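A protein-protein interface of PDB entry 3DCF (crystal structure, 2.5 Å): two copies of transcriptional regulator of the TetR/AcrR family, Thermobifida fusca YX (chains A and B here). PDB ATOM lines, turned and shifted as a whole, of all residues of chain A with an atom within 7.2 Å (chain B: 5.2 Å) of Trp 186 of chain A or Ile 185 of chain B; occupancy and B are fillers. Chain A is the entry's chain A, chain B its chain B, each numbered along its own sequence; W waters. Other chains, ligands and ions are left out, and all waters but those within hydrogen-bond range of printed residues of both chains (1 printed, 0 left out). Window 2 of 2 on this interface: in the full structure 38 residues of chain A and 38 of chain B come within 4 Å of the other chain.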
ATOM      1  N   ILE A 119      11.551 -19.898  -3.608  1.00  0.00           N
ATOM      2  CA  ILE A 119      10.180 -20.465  -3.585  1.00  0.00           C
ATOM      3  C   ILE A 119       9.134 -19.395  -3.970  1.00  0.00           C
ATOM      4  O   ILE A 119       8.338 -19.612  -4.901  1.00  0.00           O
ATOM      5  CB  ILE A 119       9.769 -21.107  -2.201  1.00  0.00           C
ATOM      6  CG1 ILE A 119      10.668 -22.287  -1.785  1.00  0.00           C
ATOM      7  CG2 ILE A 119       8.329 -21.604  -2.234  1.00  0.00           C
ATOM      8  CD1 ILE A 119      10.749 -23.427  -2.759  1.00  0.00           C
ATOM      9  N   LEU A 181      13.630 -26.899   5.766  1.00  0.00           N
ATOM     10  CA  LEU A 181      13.318 -26.786   4.327  1.00  0.00           C
ATOM     11  C   LEU A 181      11.811 -26.932   4.116  1.00  0.00           C
ATOM     12  O   LEU A 181      11.235 -26.171   3.356  1.00  0.00           O
ATOM     13  CB  LEU A 181      14.081 -27.821   3.484  1.00  0.00           C
ATOM     14  CG  LEU A 181      15.608 -27.684   3.347  1.00  0.00           C
ATOM     15  CD1 LEU A 181      16.166 -28.877   2.598  1.00  0.00           C
ATOM     16  CD2 LEU A 181      16.024 -26.353   2.655  1.00  0.00           C
ATOM     17  N   GLY A 182      11.188 -27.896   4.804  1.00  0.00           N
ATOM     18  CA  GLY A 182       9.735 -28.112   4.770  1.00  0.00           C
ATOM     19  C   GLY A 182       8.930 -26.871   5.128  1.00  0.00           C
ATOM     20  O   GLY A 182       7.924 -26.578   4.470  1.00  0.00           O
ATOM     21  N   ALA A 183       9.376 -26.156   6.173  1.00  0.00           N
ATOM     22  CA  ALA A 183       8.751 -24.888   6.620  1.00  0.00           C
ATOM     23  C   ALA A 183       8.845 -23.804   5.535  1.00  0.00           C
ATOM     24  O   ALA A 183       7.904 -23.040   5.347  1.00  0.00           O
ATOM     25  CB  ALA A 183       9.383 -24.382   7.939  1.00  0.00           C
ATOM     26  N   ALA A 184       9.982 -23.752   4.835  1.00  0.00           N
ATOM     27  CA  ALA A 184      10.205 -22.814   3.721  1.00  0.00           C
ATOM     28  C   ALA A 184       9.342 -23.159   2.498  1.00  0.00           C
ATOM     29  O   ALA A 184       8.721 -22.274   1.915  1.00  0.00           O
ATOM     30  CB  ALA A 184      11.683 -22.793   3.324  1.00  0.00           C
ATOM     31  N   ILE A 185       9.305 -24.447   2.138  1.00  0.00           N
ATOM     32  CA  ILE A 185       8.543 -24.956   0.977  1.00  0.00           C
ATOM     33  C   ILE A 185       7.018 -24.757   1.106  1.00  0.00           C
ATOM     34  O   ILE A 185       6.382 -24.308   0.161  1.00  0.00           O
ATOM     35  CB  ILE A 185       8.873 -26.465   0.703  1.00  0.00           C
ATOM     36  CG1 ILE A 185      10.343 -26.645   0.281  1.00  0.00           C
ATOM     37  CG2 ILE A 185       7.965 -27.046  -0.404  1.00  0.00           C
ATOM     38  CD1 ILE A 185      10.879 -28.066   0.408  1.00  0.00           C
ATOM     39  N   TRP A 186       6.457 -25.027   2.283  1.00  0.00           N
ATOM     40  CA  TRP A 186       4.983 -24.932   2.542  1.00  0.00           C
ATOM     41  C   TRP A 186       4.330 -23.591   2.166  1.00  0.00           C
ATOM     42  O   TRP A 186       3.115 -23.524   1.946  1.00  0.00           O
ATOM     43  CB  TRP A 186       4.675 -25.269   4.004  1.00  0.00           C
ATOM     44  CG  TRP A 186       3.247 -25.614   4.294  1.00  0.00           C
ATOM     45  CD1 TRP A 186       2.351 -24.887   5.030  1.00  0.00           C
ATOM     46  CD2 TRP A 186       2.552 -26.789   3.858  1.00  0.00           C
ATOM     47  NE1 TRP A 186       1.140 -25.545   5.086  1.00  0.00           N
ATOM     48  CE2 TRP A 186       1.231 -26.710   4.373  1.00  0.00           C
ATOM     49  CE3 TRP A 186       2.917 -27.906   3.075  1.00  0.00           C
ATOM     50  CZ2 TRP A 186       0.266 -27.709   4.136  1.00  0.00           C
ATOM     51  CZ3 TRP A 186       1.950 -28.912   2.834  1.00  0.00           C
ATOM     52  CH2 TRP A 186       0.641 -28.801   3.371  1.00  0.00           C
ATOM     53  N   THR A 187       5.144 -22.529   2.102  1.00  0.00           N
ATOM     54  CA  THR A 187       4.715 -21.212   1.610  1.00  0.00           C
ATOM     55  C   THR A 187       3.982 -21.275   0.256  1.00  0.00           C
ATOM     56  O   THR A 187       3.089 -20.448   0.034  1.00  0.00           O
ATOM     57  CB  THR A 187       5.902 -20.240   1.472  1.00  0.00           C
ATOM     58  OG1 THR A 187       6.882 -20.812   0.605  1.00  0.00           O
ATOM     59  CG2 THR A 187       6.555 -19.938   2.827  1.00  0.00           C
ATOM     60  N   TYR A 188       4.321 -22.242  -0.621  1.00  0.00           N
ATOM     61  CA  TYR A 188       3.643 -22.361  -1.934  1.00  0.00           C
ATOM     62  C   TYR A 188       2.139 -22.652  -1.810  1.00  0.00           C
ATOM     63  O   TYR A 188       1.380 -22.268  -2.689  1.00  0.00           O
ATOM     64  CB  TYR A 188       4.343 -23.338  -2.925  1.00  0.00           C
ATOM     65  CG  TYR A 188       3.973 -24.826  -2.868  1.00  0.00           C
ATOM     66  CD1 TYR A 188       2.828 -25.325  -3.538  1.00  0.00           C
ATOM     67  CD2 TYR A 188       4.800 -25.753  -2.213  1.00  0.00           C
ATOM     68  CE1 TYR A 188       2.501 -26.714  -3.505  1.00  0.00           C
ATOM     69  CE2 TYR A 188       4.488 -27.133  -2.181  1.00  0.00           C
ATOM     70  CZ  TYR A 188       3.350 -27.605  -2.829  1.00  0.00           C
ATOM     71  OH  TYR A 188       3.088 -28.949  -2.767  1.00  0.00           O
ATOM     72  N   ARG A 189       1.724 -23.324  -0.732  1.00  0.00           N
ATOM     73  CA  ARG A 189       0.298 -23.603  -0.481  1.00  0.00           C
ATOM     74  C   ARG A 189      -0.477 -22.451   0.174  1.00  0.00           C
ATOM     75  O   ARG A 189      -1.683 -22.359  -0.062  1.00  0.00           O
ATOM     76  CB  ARG A 189       0.093 -24.906   0.319  1.00  0.00           C
ATOM     77  CG  ARG A 189       0.336 -26.191  -0.505  1.00  0.00           C
ATOM     78  CD  ARG A 189      -0.318 -27.424   0.131  1.00  0.00           C
ATOM     79  NE  ARG A 189      -1.801 -27.477   0.065  1.00  0.00           N
ATOM     80  CZ  ARG A 189      -2.685 -27.099   1.011  1.00  0.00           C
ATOM     81  NH1 ARG A 189      -2.310 -26.580   2.184  1.00  0.00           N
ATOM     82  NH2 ARG A 189      -3.996 -27.246   0.775  1.00  0.00           N
ATOM     83  N   TRP A 190       0.189 -21.580   0.952  1.00  0.00           N
ATOM     84  CA  TRP A 190      -0.491 -20.456   1.651  1.00  0.00           C
ATOM     85  C   TRP A 190      -0.161 -19.006   1.216  1.00  0.00           C
ATOM     86  O   TRP A 190      -1.030 -18.137   1.367  1.00  0.00           O
ATOM     87  CB  TRP A 190      -0.348 -20.585   3.180  1.00  0.00           C
ATOM     88  CG  TRP A 190       1.023 -20.367   3.748  1.00  0.00           C
ATOM     89  CD1 TRP A 190       1.929 -21.323   4.061  1.00  0.00           C
ATOM     90  CD2 TRP A 190       1.625 -19.110   4.097  1.00  0.00           C
ATOM     91  NE1 TRP A 190       3.061 -20.752   4.583  1.00  0.00           N
ATOM     92  CE2 TRP A 190       2.908 -19.394   4.614  1.00  0.00           C
ATOM     93  CE3 TRP A 190       1.202 -17.766   4.029  1.00  0.00           C
ATOM     94  CZ2 TRP A 190       3.785 -18.387   5.062  1.00  0.00           C
ATOM     95  CZ3 TRP A 190       2.079 -16.755   4.470  1.00  0.00           C
ATOM     96  CH2 TRP A 190       3.356 -17.079   4.980  1.00  0.00           C
ATOM     97  N   TYR A 191       1.054 -18.736   0.716  1.00  0.00           N
ATOM     98  CA  TYR A 191       1.442 -17.362   0.312  1.00  0.00           C
ATOM     99  C   TYR A 191       0.593 -16.787  -0.854  1.00  0.00           C
ATOM    100  O   TYR A 191       0.492 -17.404  -1.921  1.00  0.00           O
ATOM    101  CB  TYR A 191       2.937 -17.253  -0.027  1.00  0.00           C
ATOM    102  CG  TYR A 191       3.363 -15.862  -0.503  1.00  0.00           C
ATOM    103  CD1 TYR A 191       3.346 -14.753   0.368  1.00  0.00           C
ATOM    104  CD2 TYR A 191       3.785 -15.649  -1.826  1.00  0.00           C
ATOM    105  CE1 TYR A 191       3.737 -13.453  -0.073  1.00  0.00           C
ATOM    106  CE2 TYR A 191       4.181 -14.356  -2.280  1.00  0.00           C
ATOM    107  CZ  TYR A 191       4.157 -13.267  -1.400  1.00  0.00           C
ATOM    108  OH  TYR A 191       4.552 -12.025  -1.865  1.00  0.00           O
ATOM    109  N   HIS B 115      -0.773 -32.323  16.941  1.00  0.00           N
ATOM    110  CA  HIS B 115      -0.926 -32.211  15.484  1.00  0.00           C
ATOM    111  C   HIS B 115       0.046 -33.140  14.725  1.00  0.00           C
ATOM    112  O   HIS B 115      -0.385 -33.901  13.850  1.00  0.00           O
ATOM    113  CB  HIS B 115      -0.785 -30.740  15.034  1.00  0.00           C
ATOM    114  CG  HIS B 115      -1.074 -30.521  13.584  1.00  0.00           C
ATOM    115  ND1 HIS B 115      -2.345 -30.612  13.062  1.00  0.00           N
ATOM    116  CD2 HIS B 115      -0.257 -30.211  12.550  1.00  0.00           C
ATOM    117  CE1 HIS B 115      -2.296 -30.389  11.761  1.00  0.00           C
ATOM    118  NE2 HIS B 115      -1.040 -30.143  11.426  1.00  0.00           N
ATOM    119  N   ILE B 119      -0.513 -36.543  12.498  1.00  0.00           N
ATOM    120  CA  ILE B 119       0.019 -36.681  11.120  1.00  0.00           C
ATOM    121  C   ILE B 119       0.722 -38.043  10.935  1.00  0.00           C
ATOM    122  O   ILE B 119       0.377 -38.803  10.010  1.00  0.00           O
ATOM    123  CB  ILE B 119       1.017 -35.540  10.698  1.00  0.00           C
ATOM    124  CG1 ILE B 119       0.377 -34.154  10.724  1.00  0.00           C
ATOM    125  CG2 ILE B 119       1.553 -35.771   9.296  1.00  0.00           C
ATOM    126  CD1 ILE B 119      -0.863 -33.999   9.889  1.00  0.00           C
ATOM    127  N   TYR B 130      -4.109 -33.610   0.851  1.00  0.00           N
ATOM    128  CA  TYR B 130      -3.401 -32.536   0.084  1.00  0.00           C
ATOM    129  C   TYR B 130      -3.065 -32.763  -1.413  1.00  0.00           C
ATOM    130  O   TYR B 130      -2.735 -31.787  -2.102  1.00  0.00           O
ATOM    131  CB  TYR B 130      -2.121 -32.125   0.840  1.00  0.00           C
ATOM    132  CG  TYR B 130      -2.390 -31.561   2.226  1.00  0.00           C
ATOM    133  CD1 TYR B 130      -2.983 -30.301   2.384  1.00  0.00           C
ATOM    134  CD2 TYR B 130      -2.037 -32.274   3.386  1.00  0.00           C
ATOM    135  CE1 TYR B 130      -3.234 -29.763   3.663  1.00  0.00           C
ATOM    136  CE2 TYR B 130      -2.282 -31.749   4.670  1.00  0.00           C
ATOM    137  CZ  TYR B 130      -2.879 -30.494   4.798  1.00  0.00           C
ATOM    138  OH  TYR B 130      -3.116 -29.981   6.051  1.00  0.00           O
ATOM    139  N   ALA B 178       1.029 -20.824   9.907  1.00  0.00           N
ATOM    140  CA  ALA B 178       1.243 -21.608   8.660  1.00  0.00           C
ATOM    141  C   ALA B 178       2.632 -22.270   8.577  1.00  0.00           C
ATOM    142  O   ALA B 178       2.781 -23.353   7.999  1.00  0.00           O
ATOM    143  CB  ALA B 178       1.021 -20.739   7.419  1.00  0.00           C
ATOM    144  N   LEU B 181       2.673 -25.109  11.645  1.00  0.00           N
ATOM    145  CA  LEU B 181       1.800 -26.217  11.194  1.00  0.00           C
ATOM    146  C   LEU B 181       2.384 -26.865   9.933  1.00  0.00           C
ATOM    147  O   LEU B 181       2.410 -28.084   9.833  1.00  0.00           O
ATOM    148  CB  LEU B 181       0.353 -25.752  10.934  1.00  0.00           C
ATOM    149  CG  LEU B 181      -0.537 -25.333  12.114  1.00  0.00           C
ATOM    150  CD1 LEU B 181      -1.890 -24.830  11.566  1.00  0.00           C
ATOM    151  CD2 LEU B 181      -0.762 -26.456  13.122  1.00  0.00           C
ATOM    152  N   GLY B 182       2.847 -26.032   8.993  1.00  0.00           N
ATOM    153  CA  GLY B 182       3.523 -26.475   7.758  1.00  0.00           C
ATOM    154  C   GLY B 182       4.717 -27.382   8.018  1.00  0.00           C
ATOM    155  O   GLY B 182       4.882 -28.389   7.317  1.00  0.00           O
ATOM    156  N   ALA B 183       5.539 -27.021   9.020  1.00  0.00           N
ATOM    157  CA  ALA B 183       6.707 -27.828   9.453  1.00  0.00           C
ATOM    158  C   ALA B 183       6.285 -29.212   9.967  1.00  0.00           C
ATOM    159  O   ALA B 183       6.978 -30.193   9.720  1.00  0.00           O
ATOM    160  CB  ALA B 183       7.528 -27.094  10.530  1.00  0.00           C
ATOM    161  N   ALA B 184       5.159 -29.268  10.684  1.00  0.00           N
ATOM    162  CA  ALA B 184       4.589 -30.512  11.210  1.00  0.00           C
ATOM    163  C   ALA B 184       4.004 -31.384  10.090  1.00  0.00           C
ATOM    164  O   ALA B 184       4.279 -32.581  10.036  1.00  0.00           O
ATOM    165  CB  ALA B 184       3.515 -30.197  12.248  1.00  0.00           C
ATOM    166  N   ILE B 185       3.222 -30.767   9.195  1.00  0.00           N
ATOM    167  CA  ILE B 185       2.553 -31.444   8.044  1.00  0.00           C
ATOM    168  C   ILE B 185       3.531 -32.080   7.041  1.00  0.00           C
ATOM    169  O   ILE B 185       3.306 -33.208   6.628  1.00  0.00           O
ATOM    170  CB  ILE B 185       1.594 -30.461   7.261  1.00  0.00           C
ATOM    171  CG1 ILE B 185       0.413 -30.016   8.133  1.00  0.00           C
ATOM    172  CG2 ILE B 185       1.034 -31.111   5.974  1.00  0.00           C
ATOM    173  CD1 ILE B 185      -0.287 -28.768   7.629  1.00  0.00           C
ATOM    174  N   TRP B 186       4.623 -31.378   6.697  1.00  0.00           N
ATOM    175  CA  TRP B 186       5.656 -31.847   5.709  1.00  0.00           C
ATOM    176  C   TRP B 186       6.243 -33.252   5.970  1.00  0.00           C
ATOM    177  O   TRP B 186       6.752 -33.900   5.048  1.00  0.00           O
ATOM    178  CB  TRP B 186       6.792 -30.815   5.591  1.00  0.00           C
ATOM    179  CG  TRP B 186       7.640 -30.946   4.368  1.00  0.00           C
ATOM    180  CD1 TRP B 186       8.955 -31.340   4.304  1.00  0.00           C
ATOM    181  CD2 TRP B 186       7.226 -30.692   3.021  1.00  0.00           C
ATOM    182  NE1 TRP B 186       9.389 -31.327   2.994  1.00  0.00           N
ATOM    183  CE2 TRP B 186       8.353 -30.937   2.186  1.00  0.00           C
ATOM    184  CE3 TRP B 186       6.011 -30.282   2.433  1.00  0.00           C
ATOM    185  CZ2 TRP B 186       8.306 -30.773   0.783  1.00  0.00           C
ATOM    186  CZ3 TRP B 186       5.954 -30.121   1.022  1.00  0.00           C
ATOM    187  CH2 TRP B 186       7.106 -30.361   0.219  1.00  0.00           C
ATOM    188  N   THR B 187       6.173 -33.696   7.229  1.00  0.00           N
ATOM    189  CA  THR B 187       6.539 -35.064   7.645  1.00  0.00           C
ATOM    190  C   THR B 187       5.889 -36.159   6.775  1.00  0.00           C
ATOM    191  O   THR B 187       6.505 -37.204   6.580  1.00  0.00           O
ATOM    192  CB  THR B 187       6.171 -35.350   9.137  1.00  0.00           C
ATOM    193  OG1 THR B 187       4.761 -35.152   9.333  1.00  0.00           O
ATOM    194  CG2 THR B 187       6.967 -34.456  10.111  1.00  0.00           C
ATOM    195  N   TYR B 188       4.677 -35.920   6.243  1.00  0.00           N
ATOM    196  CA  TYR B 188       4.006 -36.917   5.370  1.00  0.00           C
ATOM    197  C   TYR B 188       4.786 -37.208   4.069  1.00  0.00           C
ATOM    198  O   TYR B 188       4.623 -38.290   3.498  1.00  0.00           O
ATOM    199  CB  TYR B 188       2.502 -36.597   5.081  1.00  0.00           C
ATOM    200  CG  TYR B 188       2.155 -35.701   3.874  1.00  0.00           C
ATOM    201  CD1 TYR B 188       2.091 -36.225   2.564  1.00  0.00           C
ATOM    202  CD2 TYR B 188       1.837 -34.346   4.046  1.00  0.00           C
ATOM    203  CE1 TYR B 188       1.763 -35.402   1.455  1.00  0.00           C
ATOM    204  CE2 TYR B 188       1.500 -33.515   2.946  1.00  0.00           C
ATOM    205  CZ  TYR B 188       1.458 -34.049   1.659  1.00  0.00           C
ATOM    206  OH  TYR B 188       1.125 -33.232   0.598  1.00  0.00           O
ATOM    207  N   ARG B 189       5.589 -36.245   3.596  1.00  0.00           N
ATOM    208  CA  ARG B 189       6.430 -36.439   2.404  1.00  0.00           C
ATOM    209  C   ARG B 189       7.790 -37.101   2.672  1.00  0.00           C
ATOM    210  O   ARG B 189       8.319 -37.743   1.761  1.00  0.00           O
ATOM    211  CB  ARG B 189       6.623 -35.128   1.616  1.00  0.00           C
ATOM    212  CG  ARG B 189       5.379 -34.683   0.818  1.00  0.00           C
ATOM    213  CD  ARG B 189       5.723 -33.713  -0.320  1.00  0.00           C
ATOM    214  NE  ARG B 189       6.441 -34.292  -1.485  1.00  0.00           N
ATOM    215  CZ  ARG B 189       7.771 -34.299  -1.714  1.00  0.00           C
ATOM    216  NH1 ARG B 189       8.646 -33.768  -0.861  1.00  0.00           N
ATOM    217  NH2 ARG B 189       8.243 -34.853  -2.838  1.00  0.00           N
HETATM  218  O   HOH W   1       3.325 -31.490  -0.829  1.00  0.00           O
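Gly 182 of chain A touches Trp 186 of chain B (CA to CD1, 3.4 Å). Trp 186 of chain B touches Ile 185 of chain A (CH2 to CG2, 3.5 Å). Trp 186 of chain A touches Ala 178 of chain B. CA of Gly 182 of chain B touches CD1 of Trp 186 of chain A, 3.4 Å away. Trp 186 of chain A touches Ile 185 of chain B. CE3 of Trp 186 of chain A touches CE3 of Trp 186 of chain B, at 3.95 Å. Tyr 130 of chain B touches Arg 189 of chain A (CD1 to CZ, 3.5 Å). Trp 190 of chain A touches Ala 178 of chain B.
Of the printed residues of chain B, Trp 186 of chain A touches Ala 178 (3.4 Å), Gly 182 (3.4 Å), Ile 185 (3.5 Å) and Trp 186 (3.95 Å). Ile 185 of chain B touches just one residue of chain A: Trp 186. No residue of chain A comes within 4 Å of Ala 184 of chain B. Of the printed residues of chain A, Tyr 130 of chain B touches Arg 189. Of the printed residues of chain A, Trp 186 of chain B touches Gly 182 (3.4 Å), Ile 185 (3.5 Å) and Trp 186 (3.95 Å). His 115 of chain B touches none of the printed residues of chain A. The nearest printed residue of chain B that does not touch Trp 186 of chain A is Tyr 130 of chain B (4.003 Å). The nearest printed residue of chain B that does not touch Gly 182 of chain A is Gly 182 of chain B (4.5 Å).
Hydrophobic or aromatic side chains of chain A that line the printed part of chain B: Ile 185, Trp 186 and Trp 190. Hydrophobic or aromatic side chains of chain B within 4 Å of the printed part of chain A: Tyr 130, Ala 178, Ile 185 and Trp 186. Along chain B the printed residues that touch a printed residue of chain A span positions 130 to 186. Among the printed residues, 8 pairs touch across the chains.
Gly 182 of chain A touches Trp 186 of chain B, and with the chains exchanged Trp 186 of chain A touches Gly 182 of chain B. Ile 185 of chain A touches Trp 186 of chain B, and with the chains exchanged Trp 186 of chain A touches Ile 185 of chain B. Trp 186 of chain A touches its own counterpart, Trp 186 of chain B. Positions printed for both chains: 119, 181, 182, 183, 184, 185, 186, 187, 188 and 189. Of the 8 pairs that touch across the chains among the printed residues, 5 have their exchanged pair printed and touching as well.
Water W1 bridges OH of Tyr 188 of chain B and OH of Tyr 188 of chain A.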
